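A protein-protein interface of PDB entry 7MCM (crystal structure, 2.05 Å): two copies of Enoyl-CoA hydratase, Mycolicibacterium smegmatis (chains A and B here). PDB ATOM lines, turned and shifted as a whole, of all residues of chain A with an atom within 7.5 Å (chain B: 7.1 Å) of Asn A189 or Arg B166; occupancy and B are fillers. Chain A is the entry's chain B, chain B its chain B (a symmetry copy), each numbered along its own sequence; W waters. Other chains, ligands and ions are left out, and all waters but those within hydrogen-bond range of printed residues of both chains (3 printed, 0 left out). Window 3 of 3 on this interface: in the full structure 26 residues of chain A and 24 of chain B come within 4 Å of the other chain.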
ATOM      1  N   ASP A 129      27.486  19.743   1.014  1.00  0.00           N
ATOM      2  CA  ASP A 129      26.651  20.542   0.114  1.00  0.00           C
ATOM      3  C   ASP A 129      25.300  20.876   0.731  1.00  0.00           C
ATOM      4  O   ASP A 129      24.776  21.978   0.526  1.00  0.00           O
ATOM      5  CB  ASP A 129      26.462  19.820  -1.223  1.00  0.00           C
ATOM      6  CG  ASP A 129      27.782  19.558  -1.929  1.00  0.00           C
ATOM      7  OD1 ASP A 129      28.521  20.530  -2.185  1.00  0.00           O
ATOM      8  OD2 ASP A 129      28.102  18.388  -2.200  1.00  0.00           O
ATOM      9  N   LEU A 130      24.726  19.937   1.467  1.00  0.00           N
ATOM     10  CA  LEU A 130      23.406  20.051   2.073  1.00  0.00           C
ATOM     11  C   LEU A 130      23.511  19.510   3.482  1.00  0.00           C
ATOM     12  O   LEU A 130      24.235  18.541   3.707  1.00  0.00           O
ATOM     13  CB  LEU A 130      22.338  19.236   1.310  1.00  0.00           C
ATOM     14  CG  LEU A 130      21.996  19.677  -0.103  1.00  0.00           C
ATOM     15  CD1 LEU A 130      21.010  18.738  -0.743  1.00  0.00           C
ATOM     16  CD2 LEU A 130      21.389  21.048   0.016  1.00  0.00           C
ATOM     17  N   ARG A 131      22.788  20.122   4.422  1.00  0.00           N
ATOM     18  CA  ARG A 131      22.727  19.622   5.788  1.00  0.00           C
ATOM     19  C   ARG A 131      21.285  19.400   6.200  1.00  0.00           C
ATOM     20  O   ARG A 131      20.419  20.235   5.933  1.00  0.00           O
ATOM     21  CB  ARG A 131      23.368  20.582   6.779  1.00  0.00           C
ATOM     22  CG  ARG A 131      24.873  20.547   6.823  1.00  0.00           C
ATOM     23  CD  ARG A 131      25.404  21.928   7.229  1.00  0.00           C
ATOM     24  NE  ARG A 131      25.037  22.945   6.255  1.00  0.00           N
ATOM     25  CZ  ARG A 131      25.625  23.059   5.071  1.00  0.00           C
ATOM     26  NH1 ARG A 131      26.587  22.222   4.699  1.00  0.00           N
ATOM     27  NH2 ARG A 131      25.245  24.030   4.248  1.00  0.00           N
ATOM     28  N   ILE A 132      21.035  18.258   6.842  1.00  0.00           N
ATOM     29  CA  ILE A 132      19.821  18.023   7.607  1.00  0.00           C
ATOM     30  C   ILE A 132      20.259  17.480   8.960  1.00  0.00           C
ATOM     31  O   ILE A 132      21.362  16.943   9.105  1.00  0.00           O
ATOM     32  CB  ILE A 132      18.852  17.047   6.901  1.00  0.00           C
ATOM     33  CG1 ILE A 132      19.487  15.676   6.770  1.00  0.00           C
ATOM     34  CG2 ILE A 132      18.495  17.539   5.510  1.00  0.00           C
ATOM     35  CD1 ILE A 132      18.557  14.643   6.144  1.00  0.00           C
ATOM     36  N   ALA A 133      19.383  17.614   9.961  1.00  0.00           N
ATOM     37  CA  ALA A 133      19.783  17.330  11.336  1.00  0.00           C
ATOM     38  C   ALA A 133      18.692  16.599  12.095  1.00  0.00           C
ATOM     39  O   ALA A 133      17.498  16.783  11.839  1.00  0.00           O
ATOM     40  CB  ALA A 133      20.141  18.614  12.109  1.00  0.00           C
ATOM     41  N   ALA A 182      19.516  26.214  14.376  1.00  0.00           N
ATOM     42  CA  ALA A 182      20.204  25.901  13.127  1.00  0.00           C
ATOM     43  C   ALA A 182      19.241  25.927  11.949  1.00  0.00           C
ATOM     44  O   ALA A 182      19.572  26.453  10.884  1.00  0.00           O
ATOM     45  CB  ALA A 182      20.880  24.531  13.230  1.00  0.00           C
ATOM     46  N   LEU A 183      18.047  25.352  12.119  1.00  0.00           N
ATOM     47  CA  LEU A 183      17.039  25.397  11.065  1.00  0.00           C
ATOM     48  C   LEU A 183      16.646  26.835  10.763  1.00  0.00           C
ATOM     49  O   LEU A 183      16.635  27.256   9.604  1.00  0.00           O
ATOM     50  CB  LEU A 183      15.806  24.585  11.476  1.00  0.00           C
ATOM     51  CG  LEU A 183      14.673  24.463  10.443  1.00  0.00           C
ATOM     52  CD1 LEU A 183      15.133  23.643   9.251  1.00  0.00           C
ATOM     53  CD2 LEU A 183      13.432  23.835  11.056  1.00  0.00           C
ATOM     54  N   GLY A 186      19.124  28.625   8.674  1.00  0.00           N
ATOM     55  CA  GLY A 186      19.530  28.049   7.408  1.00  0.00           C
ATOM     56  C   GLY A 186      20.801  27.233   7.482  1.00  0.00           C
ATOM     57  O   GLY A 186      21.344  26.857   6.436  1.00  0.00           O
ATOM     58  N   LEU A 187      21.316  26.978   8.685  1.00  0.00           N
ATOM     59  CA  LEU A 187      22.461  26.081   8.810  1.00  0.00           C
ATOM     60  C   LEU A 187      22.100  24.671   8.341  1.00  0.00           C
ATOM     61  O   LEU A 187      22.930  23.987   7.733  1.00  0.00           O
ATOM     62  CB  LEU A 187      22.959  26.080  10.253  1.00  0.00           C
ATOM     63  CG  LEU A 187      24.223  25.309  10.648  1.00  0.00           C
ATOM     64  CD1 LEU A 187      25.338  25.538   9.637  1.00  0.00           C
ATOM     65  CD2 LEU A 187      24.677  25.745  12.042  1.00  0.00           C
ATOM     66  N   VAL A 188      20.855  24.241   8.580  1.00  0.00           N
ATOM     67  CA  VAL A 188      20.322  22.985   8.063  1.00  0.00           C
ATOM     68  C   VAL A 188      19.000  23.267   7.353  1.00  0.00           C
ATOM     69  O   VAL A 188      18.323  24.268   7.613  1.00  0.00           O
ATOM     70  CB  VAL A 188      20.105  21.924   9.166  1.00  0.00           C
ATOM     71  CG1 VAL A 188      21.381  21.676   9.952  1.00  0.00           C
ATOM     72  CG2 VAL A 188      18.964  22.339  10.090  1.00  0.00           C
ATOM     73  N   ASN A 189      18.638  22.359   6.441  1.00  0.00           N
ATOM     74  CA  ASN A 189      17.429  22.491   5.632  1.00  0.00           C
ATOM     75  C   ASN A 189      16.211  21.846   6.272  1.00  0.00           C
ATOM     76  O   ASN A 189      15.081  22.229   5.956  1.00  0.00           O
ATOM     77  CB  ASN A 189      17.639  21.857   4.253  1.00  0.00           C
ATOM     78  CG  ASN A 189      18.554  22.673   3.359  1.00  0.00           C
ATOM     79  OD1 ASN A 189      19.095  23.697   3.771  1.00  0.00           O
ATOM     80  ND2 ASN A 189      18.737  22.210   2.117  1.00  0.00           N
ATOM     81  N   GLU A 190      16.401  20.847   7.129  1.00  0.00           N
ATOM     82  CA  GLU A 190      15.272  20.262   7.832  1.00  0.00           C
ATOM     83  C   GLU A 190      15.773  19.580   9.097  1.00  0.00           C
ATOM     84  O   GLU A 190      16.940  19.188   9.208  1.00  0.00           O
ATOM     85  CB  GLU A 190      14.473  19.283   6.950  1.00  0.00           C
ATOM     86  CG  GLU A 190      15.279  18.197   6.289  1.00  0.00           C
ATOM     87  CD  GLU A 190      14.460  17.313   5.339  1.00  0.00           C
ATOM     88  OE1 GLU A 190      13.233  17.173   5.549  1.00  0.00           O
ATOM     89  OE2 GLU A 190      15.047  16.750   4.386  1.00  0.00           O
ATOM     90  N   VAL A 191      14.877  19.501  10.076  1.00  0.00           N
ATOM     91  CA  VAL A 191      15.150  18.871  11.360  1.00  0.00           C
ATOM     92  C   VAL A 191      14.183  17.710  11.505  1.00  0.00           C
ATOM     93  O   VAL A 191      12.969  17.886  11.349  1.00  0.00           O
ATOM     94  CB  VAL A 191      15.004  19.862  12.532  1.00  0.00           C
ATOM     95  CG1 VAL A 191      15.117  19.137  13.870  1.00  0.00           C
ATOM     96  CG2 VAL A 191      16.041  20.966  12.420  1.00  0.00           C
ATOM     97  N   LEU A 192      14.719  16.524  11.776  1.00  0.00           N
ATOM     98  CA  LEU A 192      13.929  15.310  11.860  1.00  0.00           C
ATOM     99  C   LEU A 192      14.108  14.678  13.230  1.00  0.00           C
ATOM    100  O   LEU A 192      15.111  14.907  13.914  1.00  0.00           O
ATOM    101  CB  LEU A 192      14.338  14.335  10.749  1.00  0.00           C
ATOM    102  CG  LEU A 192      14.195  15.151   9.458  1.00  0.00           C
ATOM    103  CD1 LEU A 192      15.489  15.272   8.681  1.00  0.00           C
ATOM    104  CD2 LEU A 192      13.058  14.656   8.617  1.00  0.00           C
ATOM    105  N   LEU A 204      16.134  12.491   0.356  1.00  0.00           N
ATOM    106  CA  LEU A 204      16.806  13.611  -0.296  1.00  0.00           C
ATOM    107  C   LEU A 204      17.853  13.130  -1.299  1.00  0.00           C
ATOM    108  O   LEU A 204      17.944  13.657  -2.412  1.00  0.00           O
ATOM    109  CB  LEU A 204      17.443  14.519   0.765  1.00  0.00           C
ATOM    110  CG  LEU A 204      18.180  15.767   0.268  1.00  0.00           C
ATOM    111  CD1 LEU A 204      17.263  16.656  -0.564  1.00  0.00           C
ATOM    112  CD2 LEU A 204      18.785  16.554   1.460  1.00  0.00           C
ATOM    113  N   ARG A 207      16.266  11.968  -4.517  1.00  0.00           N
ATOM    114  CA  ARG A 207      15.815  13.038  -5.408  1.00  0.00           C
ATOM    115  C   ARG A 207      16.944  13.521  -6.315  1.00  0.00           C
ATOM    116  O   ARG A 207      16.679  14.062  -7.397  1.00  0.00           O
ATOM    117  CB  ARG A 207      15.249  14.211  -4.605  1.00  0.00           C
ATOM    118  CG  ARG A 207      13.894  13.988  -3.926  1.00  0.00           C
ATOM    119  CD  ARG A 207      13.610  15.192  -2.967  1.00  0.00           C
ATOM    120  NE  ARG A 207      13.654  16.466  -3.678  1.00  0.00           N
ATOM    121  CZ  ARG A 207      13.841  17.654  -3.116  1.00  0.00           C
ATOM    122  NH1 ARG A 207      14.028  17.784  -1.815  1.00  0.00           N
ATOM    123  NH2 ARG A 207      13.833  18.742  -3.884  1.00  0.00           N
ATOM    124  N   LEU A 223      28.356  24.300  -9.906  1.00  0.00           N
ATOM    125  CA  LEU A 223      28.045  24.984  -8.650  1.00  0.00           C
ATOM    126  C   LEU A 223      29.310  25.348  -7.878  1.00  0.00           C
ATOM    127  O   LEU A 223      29.380  26.424  -7.270  1.00  0.00           O
ATOM    128  CB  LEU A 223      27.132  24.126  -7.780  1.00  0.00           C
ATOM    129  CG  LEU A 223      25.672  24.095  -8.232  1.00  0.00           C
ATOM    130  CD1 LEU A 223      24.979  22.894  -7.628  1.00  0.00           C
ATOM    131  CD2 LEU A 223      24.991  25.381  -7.830  1.00  0.00           C
ATOM    132  N   LEU B 158      21.704  31.620  -9.131  1.00  0.00           N
ATOM    133  CA  LEU B 158      20.778  30.991  -8.194  1.00  0.00           C
ATOM    134  C   LEU B 158      21.302  30.985  -6.758  1.00  0.00           C
ATOM    135  O   LEU B 158      20.517  31.300  -5.844  1.00  0.00           O
ATOM    136  CB  LEU B 158      20.427  29.569  -8.676  1.00  0.00           C
ATOM    137  CG  LEU B 158      19.323  28.856  -7.882  1.00  0.00           C
ATOM    138  CD1 LEU B 158      18.010  29.663  -7.873  1.00  0.00           C
ATOM    139  CD2 LEU B 158      19.058  27.454  -8.456  1.00  0.00           C
ATOM    140  N   PRO B 159      22.569  30.669  -6.479  1.00  0.00           N
ATOM    141  CA  PRO B 159      23.016  30.724  -5.077  1.00  0.00           C
ATOM    142  C   PRO B 159      22.927  32.114  -4.503  1.00  0.00           C
ATOM    143  O   PRO B 159      22.718  32.273  -3.291  1.00  0.00           O
ATOM    144  CB  PRO B 159      24.475  30.244  -5.142  1.00  0.00           C
ATOM    145  CG  PRO B 159      24.602  29.558  -6.420  1.00  0.00           C
ATOM    146  CD  PRO B 159      23.651  30.221  -7.366  1.00  0.00           C
ATOM    147  N   VAL B 162      19.140  32.278  -3.334  1.00  0.00           N
ATOM    148  CA  VAL B 162      18.587  31.397  -2.315  1.00  0.00           C
ATOM    149  C   VAL B 162      19.646  30.779  -1.415  1.00  0.00           C
ATOM    150  O   VAL B 162      19.306  29.977  -0.549  1.00  0.00           O
ATOM    151  CB  VAL B 162      17.703  30.294  -2.934  1.00  0.00           C
ATOM    152  CG1 VAL B 162      16.520  30.914  -3.675  1.00  0.00           C
ATOM    153  CG2 VAL B 162      18.521  29.352  -3.864  1.00  0.00           C
ATOM    154  N   GLY B 163      20.912  31.144  -1.567  1.00  0.00           N
ATOM    155  CA  GLY B 163      21.965  30.522  -0.789  1.00  0.00           C
ATOM    156  C   GLY B 163      22.445  29.240  -1.448  1.00  0.00           C
ATOM    157  O   GLY B 163      21.754  28.620  -2.251  1.00  0.00           O
ATOM    158  N   TRP B 164      23.650  28.821  -1.077  1.00  0.00           N
ATOM    159  CA  TRP B 164      24.290  27.740  -1.819  1.00  0.00           C
ATOM    160  C   TRP B 164      23.616  26.386  -1.591  1.00  0.00           C
ATOM    161  O   TRP B 164      23.557  25.568  -2.514  1.00  0.00           O
ATOM    162  CB  TRP B 164      25.774  27.658  -1.465  1.00  0.00           C
ATOM    163  CG  TRP B 164      26.555  26.970  -2.554  1.00  0.00           C
ATOM    164  CD1 TRP B 164      27.037  27.534  -3.710  1.00  0.00           C
ATOM    165  CD2 TRP B 164      26.923  25.591  -2.600  1.00  0.00           C
ATOM    166  NE1 TRP B 164      27.689  26.587  -4.461  1.00  0.00           N
ATOM    167  CE2 TRP B 164      27.636  25.388  -3.800  1.00  0.00           C
ATOM    168  CE3 TRP B 164      26.723  24.507  -1.741  1.00  0.00           C
ATOM    169  CZ2 TRP B 164      28.144  24.151  -4.159  1.00  0.00           C
ATOM    170  CZ3 TRP B 164      27.230  23.289  -2.099  1.00  0.00           C
ATOM    171  CH2 TRP B 164      27.930  23.119  -3.298  1.00  0.00           C
ATOM    172  N   ALA B 165      23.095  26.124  -0.391  1.00  0.00           N
ATOM    173  CA  ALA B 165      22.499  24.815  -0.127  1.00  0.00           C
ATOM    174  C   ALA B 165      21.190  24.639  -0.889  1.00  0.00           C
ATOM    175  O   ALA B 165      20.969  23.601  -1.528  1.00  0.00           O
ATOM    176  CB  ALA B 165      22.281  24.617   1.375  1.00  0.00           C
ATOM    177  N   ARG B 166      20.324  25.657  -0.876  1.00  0.00           N
ATOM    178  CA  ARG B 166      19.078  25.554  -1.637  1.00  0.00           C
ATOM    179  C   ARG B 166      19.345  25.539  -3.137  1.00  0.00           C
ATOM    180  O   ARG B 166      18.622  24.886  -3.890  1.00  0.00           O
ATOM    181  CB  ARG B 166      18.125  26.704  -1.293  1.00  0.00           C
ATOM    182  CG  ARG B 166      17.545  26.653   0.109  1.00  0.00           C
ATOM    183  CD  ARG B 166      16.740  25.367   0.353  1.00  0.00           C
ATOM    184  NE  ARG B 166      16.101  25.407   1.665  1.00  0.00           N
ATOM    185  CZ  ARG B 166      15.532  24.374   2.272  1.00  0.00           C
ATOM    186  NH1 ARG B 166      15.484  23.177   1.707  1.00  0.00           N
ATOM    187  NH2 ARG B 166      15.005  24.544   3.481  1.00  0.00           N
ATOM    188  N   ALA B 167      20.357  26.278  -3.600  1.00  0.00           N
ATOM    189  CA  ALA B 167      20.672  26.229  -5.025  1.00  0.00           C
ATOM    190  C   ALA B 167      21.138  24.833  -5.430  1.00  0.00           C
ATOM    191  O   ALA B 167      20.833  24.361  -6.529  1.00  0.00           O
ATOM    192  CB  ALA B 167      21.735  27.269  -5.370  1.00  0.00           C
ATOM    193  N   ALA B 168      21.912  24.179  -4.559  1.00  0.00           N
ATOM    194  CA  ALA B 168      22.326  22.805  -4.803  1.00  0.00           C
ATOM    195  C   ALA B 168      21.113  21.884  -4.853  1.00  0.00           C
ATOM    196  O   ALA B 168      20.980  21.064  -5.765  1.00  0.00           O
ATOM    197  CB  ALA B 168      23.312  22.352  -3.715  1.00  0.00           C
ATOM    198  N   GLU B 169      20.201  22.028  -3.889  1.00  0.00           N
ATOM    199  CA  GLU B 169      18.989  21.219  -3.903  1.00  0.00           C
ATOM    200  C   GLU B 169      18.214  21.408  -5.205  1.00  0.00           C
ATOM    201  O   GLU B 169      17.816  20.429  -5.847  1.00  0.00           O
ATOM    202  CB  GLU B 169      18.108  21.558  -2.701  1.00  0.00           C
ATOM    203  CG  GLU B 169      16.792  20.804  -2.717  1.00  0.00           C
ATOM    204  CD  GLU B 169      15.912  21.151  -1.544  1.00  0.00           C
ATOM    205  OE1 GLU B 169      16.401  21.827  -0.620  1.00  0.00           O
ATOM    206  OE2 GLU B 169      14.736  20.745  -1.542  1.00  0.00           O
ATOM    207  N   MET B 170      18.006  22.660  -5.629  1.00  0.00           N
ATOM    208  CA  MET B 170      17.234  22.881  -6.853  1.00  0.00           C
ATOM    209  C   MET B 170      17.971  22.362  -8.080  1.00  0.00           C
ATOM    210  O   MET B 170      17.353  21.802  -8.993  1.00  0.00           O
ATOM    211  CB  MET B 170      16.933  24.374  -7.038  1.00  0.00           C
ATOM    212  CG  MET B 170      15.986  24.964  -6.014  1.00  0.00           C
ATOM    213  SD  MET B 170      15.705  26.732  -6.238  1.00  0.00           S
ATOM    214  CE  MET B 170      14.932  26.755  -7.841  1.00  0.00           C
ATOM    215  N   THR B 171      19.284  22.570  -8.139  1.00  0.00           N
ATOM    216  CA  THR B 171      20.031  22.224  -9.342  1.00  0.00           C
ATOM    217  C   THR B 171      20.289  20.727  -9.444  1.00  0.00           C
ATOM    218  O   THR B 171      20.300  20.167 -10.546  1.00  0.00           O
ATOM    219  CB  THR B 171      21.360  22.985  -9.367  1.00  0.00           C
ATOM    220  OG1 THR B 171      21.111  24.378  -9.128  1.00  0.00           O
ATOM    221  CG2 THR B 171      22.026  22.825 -10.722  1.00  0.00           C
ATOM    222  N   LEU B 172      20.506  20.062  -8.313  1.00  0.00           N
ATOM    223  CA  LEU B 172      20.868  18.651  -8.349  1.00  0.00           C
ATOM    224  C   LEU B 172      19.661  17.730  -8.363  1.00  0.00           C
ATOM    225  O   LEU B 172      19.784  16.573  -8.802  1.00  0.00           O
ATOM    226  CB  LEU B 172      21.764  18.302  -7.149  1.00  0.00           C
ATOM    227  CG  LEU B 172      23.063  19.119  -7.024  1.00  0.00           C
ATOM    228  CD1 LEU B 172      23.763  18.818  -5.687  1.00  0.00           C
ATOM    229  CD2 LEU B 172      23.984  18.817  -8.195  1.00  0.00           C
ATOM    230  N   VAL B 177       9.748  24.042  -7.378  1.00  0.00           N
ATOM    231  CA  VAL B 177       9.627  24.814  -6.144  1.00  0.00           C
ATOM    232  C   VAL B 177       8.397  25.711  -6.296  1.00  0.00           C
ATOM    233  O   VAL B 177       8.357  26.567  -7.191  1.00  0.00           O
ATOM    234  CB  VAL B 177      10.895  25.647  -5.890  1.00  0.00           C
ATOM    235  CG1 VAL B 177      10.764  26.553  -4.640  1.00  0.00           C
ATOM    236  CG2 VAL B 177      12.122  24.735  -5.826  1.00  0.00           C
ATOM    237  N   THR B 181       7.059  28.002  -1.171  1.00  0.00           N
ATOM    238  CA  THR B 181       8.427  27.599  -0.854  1.00  0.00           C
ATOM    239  C   THR B 181       9.420  28.633  -1.361  1.00  0.00           C
ATOM    240  O   THR B 181      10.377  28.988  -0.662  1.00  0.00           O
ATOM    241  CB  THR B 181       8.728  26.226  -1.451  1.00  0.00           C
ATOM    242  OG1 THR B 181       7.712  25.298  -1.043  1.00  0.00           O
ATOM    243  CG2 THR B 181      10.079  25.731  -0.970  1.00  0.00           C
ATOM    244  N   SER B 184       9.462  31.402   1.061  1.00  0.00           N
ATOM    245  CA  SER B 184      10.166  30.979   2.267  1.00  0.00           C
ATOM    246  C   SER B 184      11.679  30.998   2.079  1.00  0.00           C
ATOM    247  O   SER B 184      12.422  31.297   3.020  1.00  0.00           O
ATOM    248  CB  SER B 184       9.689  29.583   2.666  1.00  0.00           C
ATOM    249  OG  SER B 184      10.463  29.074   3.728  1.00  0.00           O
ATOM    250  N   TRP B 185      12.156  30.660   0.885  1.00  0.00           N
ATOM    251  CA  TRP B 185      13.588  30.617   0.622  1.00  0.00           C
ATOM    252  C   TRP B 185      14.163  31.963   0.201  1.00  0.00           C
ATOM    253  O   TRP B 185      15.389  32.095   0.115  1.00  0.00           O
ATOM    254  CB  TRP B 185      13.908  29.586  -0.468  1.00  0.00           C
ATOM    255  CG  TRP B 185      13.601  28.165  -0.106  1.00  0.00           C
ATOM    256  CD1 TRP B 185      13.137  27.695   1.096  1.00  0.00           C
ATOM    257  CD2 TRP B 185      13.750  27.014  -0.959  1.00  0.00           C
ATOM    258  NE1 TRP B 185      12.993  26.322   1.042  1.00  0.00           N
ATOM    259  CE2 TRP B 185      13.359  25.884  -0.210  1.00  0.00           C
ATOM    260  CE3 TRP B 185      14.179  26.834  -2.287  1.00  0.00           C
ATOM    261  CZ2 TRP B 185      13.377  24.590  -0.746  1.00  0.00           C
ATOM    262  CZ3 TRP B 185      14.201  25.551  -2.815  1.00  0.00           C
ATOM    263  CH2 TRP B 185      13.793  24.446  -2.049  1.00  0.00           C
HETATM  264  O   HOH W   1      13.963  20.932   3.021  1.00  0.00           O
HETATM  265  O   HOH W   2      12.902  21.295  -3.865  1.00  0.00           O
HETATM  266  O   HOH W   3      17.424  19.977   1.577  1.00  0.00           O
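NH2 of Arg B166 is in hydrogen-bond range of O of Asn A189, 3.4 Å away. OE2 of Glu B169 lies within salt-bridge range of NH1 of Arg A207. The indole nitrogen of Trp B164 is in hydrogen-bond range of the backbone carbonyl oxygen of Leu A223.
The backbone carbonyl oxygen (O) of Arg A131 lies within hydrogen-bond range of the backbone NH (N) of Asn A189. The side-chain carboxylate (OE1) of Glu B169 is in salt-bridge range of the guanidinium group (NH1) of Arg B166 (2.8 Å).
Among the printed residues, merely in contact across the chains: Asp A129 with Trp B164, Leu A130 with Ala B165, Asn A189 with Glu B169, Asp A129 with Ala B165 and Leu A223 with Ala B168.
Of the printed residues of chain B, Asp A129 touches Trp B164 (2.9 Å) and Ala B165 (3.7 Å). Of the printed residues of chain B, Leu A130 touches Ala B165 (3.0 Å). Ala A133 touches none of the printed residues of chain B. Of chain B, only Arg B166 (3.4 Å) and Glu B169 (3.6 Å) come within 4 Å of Asn A189. Printed residues of chain B within 4 Å of Arg A207: Glu B169. Ala B165 touches just these residues of chain A: Asp A129 and Leu A130. Arg B166 touches just one residue of chain A: Asn A189 (3.4 Å). Of the printed residues of chain A, Ala B168 touches Leu A223. Printed residues of chain A within 4 Å of Glu B169: Asn A189 and Arg A207. The nearest residue of chain B that does not touch Asn A189 is Ala B165 (4.1 Å).
Of the 17 printed residues of chain A, 5 touch a printed residue of chain B. Hydrophobic or aromatic side chains of chain A that line the printed part of chain B: Leu A130 and Leu A223. Among the printed residues, 8 pairs touch across the chains. Among the printed residues, Asp or Glu carboxylates within 4 Å of a Lys or Arg side-chain nitrogen of the other chain: Arg A207 with Glu B169.
No position is printed for both chains.
Water W3 bridges ND2 of Asn A189 (2.6 Å) and OE1 of Glu B169 (3.0 Å). Water W2 bridges the guanidinium group of Arg A207 (2.7 Å) and the side-chain carboxylate of Glu B169 (3.0 Å). Water W1 lies within hydrogen-bond range of NH1 of Arg B166 (3.0 Å) and O of Asn A189 (3.4 Å).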
